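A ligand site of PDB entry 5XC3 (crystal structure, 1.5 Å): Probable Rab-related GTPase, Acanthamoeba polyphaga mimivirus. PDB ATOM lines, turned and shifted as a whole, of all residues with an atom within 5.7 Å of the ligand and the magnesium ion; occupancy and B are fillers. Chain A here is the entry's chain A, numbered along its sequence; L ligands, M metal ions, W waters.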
ATOM      1  N   GLY A  12      25.541  -7.625  23.240  1.00  0.00           N
ATOM      2  CA  GLY A  12      24.597  -8.540  22.625  1.00  0.00           C
ATOM      3  C   GLY A  12      23.212  -7.938  22.645  1.00  0.00           C
ATOM      4  O   GLY A  12      22.894  -7.022  23.405  1.00  0.00           O
ATOM      5  N   SER A  13      22.327  -8.485  21.799  1.00  0.00           N
ATOM      6  CA  SER A  13      21.012  -7.896  21.634  1.00  0.00           C
ATOM      7  C   SER A  13      20.135  -8.076  22.874  1.00  0.00           C
ATOM      8  O   SER A  13      20.447  -8.846  23.790  1.00  0.00           O
ATOM      9  CB  SER A  13      20.351  -8.457  20.382  1.00  0.00           C
ATOM     10  OG  SER A  13      21.227  -8.268  19.281  1.00  0.00           O
ATOM     11  N   SER A  14      19.038  -7.335  22.912  1.00  0.00           N
ATOM     12  CA  SER A  14      18.157  -7.362  24.071  1.00  0.00           C
ATOM     13  C   SER A  14      17.574  -8.753  24.285  1.00  0.00           C
ATOM     14  O   SER A  14      17.172  -9.431  23.333  1.00  0.00           O
ATOM     15  CB  SER A  14      16.993  -6.390  23.861  1.00  0.00           C
ATOM     16  OG  SER A  14      17.451  -5.064  23.755  1.00  0.00           O
ATOM     17  N   GLY A  15      17.546  -9.177  25.550  1.00  0.00           N
ATOM     18  CA  GLY A  15      16.844 -10.384  25.960  1.00  0.00           C
ATOM     19  C   GLY A  15      17.600 -11.671  25.745  1.00  0.00           C
ATOM     20  O   GLY A  15      17.019 -12.746  25.956  1.00  0.00           O
ATOM     21  N   VAL A  16      18.868 -11.616  25.356  1.00  0.00           N
ATOM     22  CA  VAL A  16      19.643 -12.828  25.107  1.00  0.00           C
ATOM     23  C   VAL A  16      20.141 -13.495  26.385  1.00  0.00           C
ATOM     24  O   VAL A  16      20.551 -14.657  26.333  1.00  0.00           O
ATOM     25  CB  VAL A  16      20.796 -12.606  24.120  1.00  0.00           C
ATOM     26  CG1 VAL A  16      20.272 -12.087  22.796  1.00  0.00           C
ATOM     27  CG2 VAL A  16      21.810 -11.628  24.689  1.00  0.00           C
ATOM     28  N   GLY A  17      20.130 -12.804  27.511  1.00  0.00           N
ATOM     29  CA  GLY A  17      20.543 -13.359  28.776  1.00  0.00           C
ATOM     30  C   GLY A  17      21.810 -12.778  29.375  1.00  0.00           C
ATOM     31  O   GLY A  17      22.397 -13.407  30.279  1.00  0.00           O
ATOM     32  N   LYS A  18      22.239 -11.595  28.922  1.00  0.00           N
ATOM     33  CA  LYS A  18      23.466 -10.988  29.438  1.00  0.00           C
ATOM     34  C   LYS A  18      23.391 -10.792  30.935  1.00  0.00           C
ATOM     35  O   LYS A  18      24.276 -11.226  31.681  1.00  0.00           O
ATOM     36  CB  LYS A  18      23.695  -9.635  28.748  1.00  0.00           C
ATOM     37  CG  LYS A  18      23.963  -9.749  27.254  1.00  0.00           C
ATOM     38  CD  LYS A  18      24.193  -8.378  26.595  1.00  0.00           C
ATOM     39  CE  LYS A  18      23.041  -7.414  26.806  1.00  0.00           C
ATOM     40  NZ  LYS A  18      21.778  -7.832  26.107  1.00  0.00           N
ATOM     41  N   SER A  19      22.334 -10.118  31.406  1.00  0.00           N
ATOM     42  CA  SER A  19      22.228  -9.872  32.843  1.00  0.00           C
ATOM     43  C   SER A  19      22.098 -11.154  33.633  1.00  0.00           C
ATOM     44  O   SER A  19      22.639 -11.279  34.734  1.00  0.00           O
ATOM     45  CB  SER A  19      21.054  -8.938  33.109  1.00  0.00           C
ATOM     46  OG  SER A  19      21.238  -7.712  32.419  1.00  0.00           O
ATOM     47  N   SER A  20      21.380 -12.142  33.087  1.00  0.00           N
ATOM     48  CA  SER A  20      21.181 -13.383  33.829  1.00  0.00           C
ATOM     49  C   SER A  20      22.487 -14.162  33.968  1.00  0.00           C
ATOM     50  O   SER A  20      22.749 -14.767  35.016  1.00  0.00           O
ATOM     51  CB  SER A  20      20.100 -14.225  33.133  1.00  0.00           C
ATOM     52  OG  SER A  20      18.871 -13.517  33.105  1.00  0.00           O
ATOM     53  N   ILE A  21      23.328 -14.144  32.934  1.00  0.00           N
ATOM     54  CA  ILE A  21      24.634 -14.770  33.036  1.00  0.00           C
ATOM     55  C   ILE A  21      25.460 -14.099  34.119  1.00  0.00           C
ATOM     56  O   ILE A  21      26.108 -14.779  34.934  1.00  0.00           O
ATOM     57  CB  ILE A  21      25.335 -14.728  31.662  1.00  0.00           C
ATOM     58  CG1 ILE A  21      24.749 -15.789  30.726  1.00  0.00           C
ATOM     59  CG2 ILE A  21      26.817 -14.946  31.807  1.00  0.00           C
ATOM     60  CD1 ILE A  21      25.129 -15.566  29.271  1.00  0.00           C
ATOM     61  N   LYS A  30      19.221 -15.201  40.298  1.00  0.00           N
ATOM     62  CA  LYS A  30      18.794 -13.945  39.715  1.00  0.00           C
ATOM     63  C   LYS A  30      18.242 -13.054  40.820  1.00  0.00           C
ATOM     64  O   LYS A  30      17.312 -13.451  41.523  1.00  0.00           O
ATOM     65  CB  LYS A  30      17.726 -14.199  38.655  1.00  0.00           C
ATOM     66  CG  LYS A  30      17.348 -12.992  37.840  1.00  0.00           C
ATOM     67  CD  LYS A  30      18.533 -12.527  37.001  1.00  0.00           C
ATOM     68  CE  LYS A  30      18.069 -11.613  35.907  1.00  0.00           C
ATOM     69  NZ  LYS A  30      17.081 -12.318  35.042  1.00  0.00           N
ATOM     70  N   ASP A  61      27.648  -4.359  32.537  1.00  0.00           N
ATOM     71  CA  ASP A  61      26.444  -4.882  31.924  1.00  0.00           C
ATOM     72  C   ASP A  61      25.592  -3.701  31.484  1.00  0.00           C
ATOM     73  O   ASP A  61      25.682  -2.605  32.043  1.00  0.00           O
ATOM     74  CB  ASP A  61      25.686  -5.773  32.923  1.00  0.00           C
ATOM     75  CG  ASP A  61      24.473  -6.468  32.317  1.00  0.00           C
ATOM     76  OD1 ASP A  61      24.466  -6.738  31.087  1.00  0.00           O
ATOM     77  OD2 ASP A  61      23.535  -6.763  33.083  1.00  0.00           O
ATOM     78  N   THR A  62      24.802  -3.903  30.436  1.00  0.00           N
ATOM     79  CA  THR A  62      23.967  -2.806  29.963  1.00  0.00           C
ATOM     80  C   THR A  62      22.768  -2.610  30.870  1.00  0.00           C
ATOM     81  O   THR A  62      22.396  -3.471  31.675  1.00  0.00           O
ATOM     82  CB  THR A  62      23.459  -3.063  28.536  1.00  0.00           C
ATOM     83  OG1 THR A  62      22.410  -4.047  28.575  1.00  0.00           O
ATOM     84  CG2 THR A  62      24.571  -3.549  27.611  1.00  0.00           C
ATOM     85  N   GLY A  64      19.824  -1.906  29.352  1.00  0.00           N
ATOM     86  CA  GLY A  64      18.796  -1.970  28.324  1.00  0.00           C
ATOM     87  C   GLY A  64      19.049  -1.132  27.098  1.00  0.00           C
ATOM     88  O   GLY A  64      18.271  -1.211  26.142  1.00  0.00           O
ATOM     89  N   GLU A  66      21.029  -1.438  24.687  1.00  0.00           N
ATOM     90  CA  GLU A  66      21.301  -2.179  23.458  1.00  0.00           C
ATOM     91  C   GLU A  66      20.071  -2.317  22.566  1.00  0.00           C
ATOM     92  O   GLU A  66      20.227  -2.581  21.373  1.00  0.00           O
ATOM     93  CB  GLU A  66      21.896  -3.558  23.779  1.00  0.00           C
ATOM     94  CG  GLU A  66      20.899  -4.553  24.366  1.00  0.00           C
ATOM     95  CD  GLU A  66      20.787  -4.460  25.885  1.00  0.00           C
ATOM     96  OE1 GLU A  66      20.347  -5.456  26.498  1.00  0.00           O
ATOM     97  OE2 GLU A  66      21.105  -3.400  26.463  1.00  0.00           O
ATOM     98  N   ASN A 119      23.812 -18.714  24.167  1.00  0.00           N
ATOM     99  CA  ASN A 119      23.073 -18.869  25.401  1.00  0.00           C
ATOM    100  C   ASN A 119      21.699 -19.499  25.174  1.00  0.00           C
ATOM    101  O   ASN A 119      21.176 -19.538  24.046  1.00  0.00           O
ATOM    102  CB  ASN A 119      22.911 -17.520  26.106  1.00  0.00           C
ATOM    103  CG  ASN A 119      22.541 -17.656  27.569  1.00  0.00           C
ATOM    104  OD1 ASN A 119      22.967 -18.597  28.241  1.00  0.00           O
ATOM    105  ND2 ASN A 119      21.748 -16.722  28.077  1.00  0.00           N
ATOM    106  N   LYS A 120      21.122 -19.980  26.282  1.00  0.00           N
ATOM    107  CA  LYS A 120      19.787 -20.579  26.379  1.00  0.00           C
ATOM    108  C   LYS A 120      19.743 -22.020  25.869  1.00  0.00           C
ATOM    109  O   LYS A 120      18.701 -22.470  25.383  1.00  0.00           O
ATOM    110  CB  LYS A 120      18.686 -19.711  25.740  1.00  0.00           C
ATOM    111  CG  LYS A 120      18.666 -18.259  26.219  1.00  0.00           C
ATOM    112  CD  LYS A 120      17.317 -17.584  26.012  1.00  0.00           C
ATOM    113  CE  LYS A 120      17.430 -16.089  26.315  1.00  0.00           C
ATOM    114  NZ  LYS A 120      16.115 -15.401  26.177  1.00  0.00           N
ATOM    115  N   ILE A 121      20.836 -22.767  26.041  1.00  0.00           N
ATOM    116  CA  ILE A 121      20.881 -24.157  25.600  1.00  0.00           C
ATOM    117  C   ILE A 121      19.949 -25.064  26.401  1.00  0.00           C
ATOM    118  O   ILE A 121      19.790 -26.227  26.031  1.00  0.00           O
ATOM    119  CB  ILE A 121      22.310 -24.718  25.572  1.00  0.00           C
ATOM    120  CG1 ILE A 121      22.889 -24.803  26.979  1.00  0.00           C
ATOM    121  CG2 ILE A 121      23.188 -23.845  24.672  1.00  0.00           C
ATOM    122  CD1 ILE A 121      24.321 -25.333  27.045  1.00  0.00           C
ATOM    123  N   ASP A 122      19.352 -24.561  27.490  1.00  0.00           N
ATOM    124  CA  ASP A 122      18.336 -25.329  28.202  1.00  0.00           C
ATOM    125  C   ASP A 122      17.079 -25.539  27.380  1.00  0.00           C
ATOM    126  O   ASP A 122      16.293 -26.441  27.704  1.00  0.00           O
ATOM    127  CB  ASP A 122      17.950 -24.607  29.494  1.00  0.00           C
ATOM    128  CG  ASP A 122      17.487 -23.194  29.239  1.00  0.00           C
ATOM    129  OD1 ASP A 122      18.350 -22.333  28.941  1.00  0.00           O
ATOM    130  OD2 ASP A 122      16.269 -22.932  29.316  1.00  0.00           O
ATOM    131  N   ILE A 123      16.844 -24.715  26.369  1.00  0.00           N
ATOM    132  CA  ILE A 123      15.636 -24.819  25.570  1.00  0.00           C
ATOM    133  C   ILE A 123      15.750 -25.998  24.629  1.00  0.00           C
ATOM    134  O   ILE A 123      16.840 -26.302  24.121  1.00  0.00           O
ATOM    135  CB  ILE A 123      15.400 -23.504  24.810  1.00  0.00           C
ATOM    136  CG1 ILE A 123      15.273 -22.350  25.797  1.00  0.00           C
ATOM    137  CG2 ILE A 123      14.164 -23.608  23.892  1.00  0.00           C
ATOM    138  CD1 ILE A 123      14.962 -21.017  25.146  1.00  0.00           C
ATOM    139  N   ALA A 149      26.152 -21.997  26.541  1.00  0.00           N
ATOM    140  CA  ALA A 149      25.827 -21.791  27.953  1.00  0.00           C
ATOM    141  C   ALA A 149      24.319 -21.712  28.170  1.00  0.00           C
ATOM    142  O   ALA A 149      23.533 -21.554  27.231  1.00  0.00           O
ATOM    143  CB  ALA A 149      26.504 -20.534  28.514  1.00  0.00           C
ATOM    144  N   SER A 150      23.932 -21.833  29.441  1.00  0.00           N
ATOM    145  CA  SER A 150      22.606 -21.445  29.898  1.00  0.00           C
ATOM    146  C   SER A 150      22.785 -20.771  31.248  1.00  0.00           C
ATOM    147  O   SER A 150      23.525 -21.273  32.103  1.00  0.00           O
ATOM    148  CB  SER A 150      21.686 -22.664  30.073  1.00  0.00           C
ATOM    149  OG  SER A 150      20.536 -22.314  30.813  1.00  0.00           O
ATOM    150  N   SER A 151      22.105 -19.633  31.436  1.00  0.00           N
ATOM    151  CA  SER A 151      22.180 -18.963  32.731  1.00  0.00           C
ATOM    152  C   SER A 151      21.632 -19.842  33.853  1.00  0.00           C
ATOM    153  O   SER A 151      21.898 -19.568  35.029  1.00  0.00           O
ATOM    154  CB  SER A 151      21.442 -17.629  32.721  1.00  0.00           C
ATOM    155  OG  SER A 151      21.629 -16.907  31.513  1.00  0.00           O
ATOM    156  N   PHE A 152      20.866 -20.885  33.522  1.00  0.00           N
ATOM    157  CA  PHE A 152      20.301 -21.797  34.508  1.00  0.00           C
ATOM    158  C   PHE A 152      21.203 -22.986  34.792  1.00  0.00           C
ATOM    159  O   PHE A 152      20.872 -23.802  35.669  1.00  0.00           O
ATOM    160  CB  PHE A 152      18.932 -22.291  34.032  1.00  0.00           C
ATOM    161  CG  PHE A 152      17.959 -21.197  33.723  1.00  0.00           C
ATOM    162  CD1 PHE A 152      17.863 -20.079  34.542  1.00  0.00           C
ATOM    163  CD2 PHE A 152      17.138 -21.268  32.608  1.00  0.00           C
ATOM    164  CE1 PHE A 152      16.952 -19.067  34.251  1.00  0.00           C
ATOM    165  CE2 PHE A 152      16.226 -20.256  32.317  1.00  0.00           C
ATOM    166  CZ  PHE A 152      16.142 -19.155  33.126  1.00  0.00           C
HETATM  167  P1  LIG L   1      19.510  -9.267  28.610  1.00  0.00           P
HETATM  168  O1  LIG L   1      20.417  -9.809  27.562  1.00  0.00           O
HETATM  169  O2  LIG L   1      20.197  -8.690  29.834  1.00  0.00           O
HETATM  170  O3  LIG L   1      18.494  -8.327  28.018  1.00  0.00           O
HETATM  171  O4  LIG L   1      18.684 -10.584  29.083  1.00  0.00           O
HETATM  172  P2  LIG L   1      18.120 -10.965  30.531  1.00  0.00           P
HETATM  173  O5  LIG L   1      19.229 -11.508  31.396  1.00  0.00           O
HETATM  174  O6  LIG L   1      17.377  -9.804  31.132  1.00  0.00           O
HETATM  175  O7  LIG L   1      17.152 -12.195  30.180  1.00  0.00           O
HETATM  176  C1  LIG L   1      15.958 -11.965  29.431  1.00  0.00           C
HETATM  177  C2  LIG L   1      15.001 -13.099  29.787  1.00  0.00           C
HETATM  178  O8  LIG L   1      15.551 -14.343  29.317  1.00  0.00           O
HETATM  179  C3  LIG L   1      14.807 -13.259  31.282  1.00  0.00           C
HETATM  180  O9  LIG L   1      13.450 -13.681  31.492  1.00  0.00           O
HETATM  181  C4  LIG L   1      15.747 -14.376  31.653  1.00  0.00           C
HETATM  182  O10 LIG L   1      15.417 -15.084  32.853  1.00  0.00           O
HETATM  183  C5  LIG L   1      15.668 -15.235  30.401  1.00  0.00           C
HETATM  184  N1  LIG L   1      16.906 -16.009  30.294  1.00  0.00           N
HETATM  185  C6  LIG L   1      18.177 -15.594  30.553  1.00  0.00           C
HETATM  186  N2  LIG L   1      19.060 -16.590  30.339  1.00  0.00           N
HETATM  187  C7  LIG L   1      18.356 -17.680  29.955  1.00  0.00           C
HETATM  188  C8  LIG L   1      18.670 -19.074  29.588  1.00  0.00           C
HETATM  189  O11 LIG L   1      19.843 -19.508  29.578  1.00  0.00           O
HETATM  190  N3  LIG L   1      17.639 -19.865  29.247  1.00  0.00           N
HETATM  191  C9  LIG L   1      16.361 -19.420  29.220  1.00  0.00           C
HETATM  192  N4  LIG L   1      15.380 -20.282  28.872  1.00  0.00           N
HETATM  193  N5  LIG L   1      16.001 -18.167  29.546  1.00  0.00           N
HETATM  194  C10 LIG L   1      16.950 -17.273  29.915  1.00  0.00           C
HETATM  195 MG    MG M   1      20.240  -6.911  30.745  1.00  0.00          MG
HETATM  196  O   HOH W   1      12.236 -14.969  29.070  1.00  0.00           O
HETATM  197  O   HOH W   2      20.151  -5.148  31.756  1.00  0.00           O
HETATM  198  O   HOH W   3      19.301  -6.009  29.080  1.00  0.00           O
HETATM  199  O   HOH W   4      14.119 -16.915  27.719  1.00  0.00           O
HETATM  200  O   HOH W   5      15.876  -7.942  28.757  1.00  0.00           O
HETATM  201  O   HOH W   6      16.593  -9.974  33.643  1.00  0.00           O
HETATM  202  O   HOH W   7      22.075  -6.400  30.034  1.00  0.00           O
HETATM  203  O   HOH W   8      18.395  -7.356  31.569  1.00  0.00           O
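N of Ser 19 lies within hydrogen-bond range of O5 of the ligand, at 3.4 Å. OD1 of Asp 122 lies within hydrogen-bond range of N3 of the ligand. The backbone NH of Ser 20 is in hydrogen-bond range of an oxygen (O5) of the ligand (2.8 Å). OG of Ser 20 is in hydrogen-bond range of O5 of the ligand (2.7 Å). The backbone NH of Gly 15 lies within hydrogen-bond range of an oxygen (O3) of the ligand (2.8 Å). The backbone NH (N) of Lys 18 is in hydrogen-bond range of an oxygen (O1) of the ligand, 2.9 Å away. NZ of Lys 18 is in salt-bridge range of O1 of the ligand (2.8 Å). N of Ser 151 lies within hydrogen-bond range of O11 of the ligand. A nitrogen (N2) of the ligand lies within hydrogen-bond range of the side-chain hydroxyl (OG) of Ser 151. O1 of the ligand lies within hydrogen-bond range of N of Gly 17, 3.0 Å away. An oxygen (O11) of the ligand lies within hydrogen-bond range of the side-chain hydroxyl of Ser 150 (3.1 Å). An oxygen (O1) of the ligand is in hydrogen-bond range of the backbone NH (N) of Val 16 (3.2 Å). The side-chain amino group (NZ) of Lys 120 is in hydrogen-bond range of an oxygen (O8) of the ligand.
OG of Ser 19 sits close to OD2 of Asp 61. OG of Ser 150 is in hydrogen-bond range of OD1 of Asp 122. OE1 of Glu 66 lies within salt-bridge range of NZ of Lys 18, 2.8 Å away. OG of Ser 150 lies close to N of Phe 152 (3.1 Å). O of Val 16 lies within hydrogen-bond range of ND2 of Asn 119 (3.0 Å). The backbone NH of Lys 120 lies within hydrogen-bond range of the backbone carbonyl oxygen of Ala 149 (3.0 Å). The side-chain carboxylate (OE2) of Glu 66 lies within hydrogen-bond range of the side-chain hydroxyl (OG1) of Thr 62 (2.6 Å). N of Gly 64 sits close to OE2 of Glu 66 (3.5 Å).
Ser 13 touches the ligand (O to O1, 3.9 Å). Ser 14 touches the ligand (C to O3, 3.9 Å). NZ of Lys 30 touches O10 of the ligand, 3.9 Å away. OE1 of Glu 66 touches O3 of the ligand, 3.7 Å away. Asn 119 touches the ligand. Ile 123 touches the ligand. CE2 of Phe 152 touches C9 of the ligand, 3.2 Å away. The nearest printed residue that does not touch the ligand is Ala 149 (4.8 Å).
One residue has an atom within 4 Å of the magnesium ion: Ser 19.
The magnesium ion is bound by O2 of the ligand (2.0 Å), water W7 (2.0 Å), water W2 (2.0 Å), water W8 (2.1 Å), OG of Ser 19 (2.1 Å) and water W3 (2.1 Å).
Water W3 bridges an oxygen (O3) of the ligand (2.7 Å) and the side-chain carboxylate (OE1) of Glu 66 (2.8 Å). Water W7 bridges the side-chain carboxylate (OD1) of Asp 61 (2.6 Å) and the side-chain hydroxyl (OG1) of Thr 62 (2.8 Å). Water W6 lies within hydrogen-bond range of O6 of the ligand (2.6 Å) and NZ of Lys 30 (2.8 Å). Water W4 lies within hydrogen-bond range of N5 of the ligand and NZ of Lys 120.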
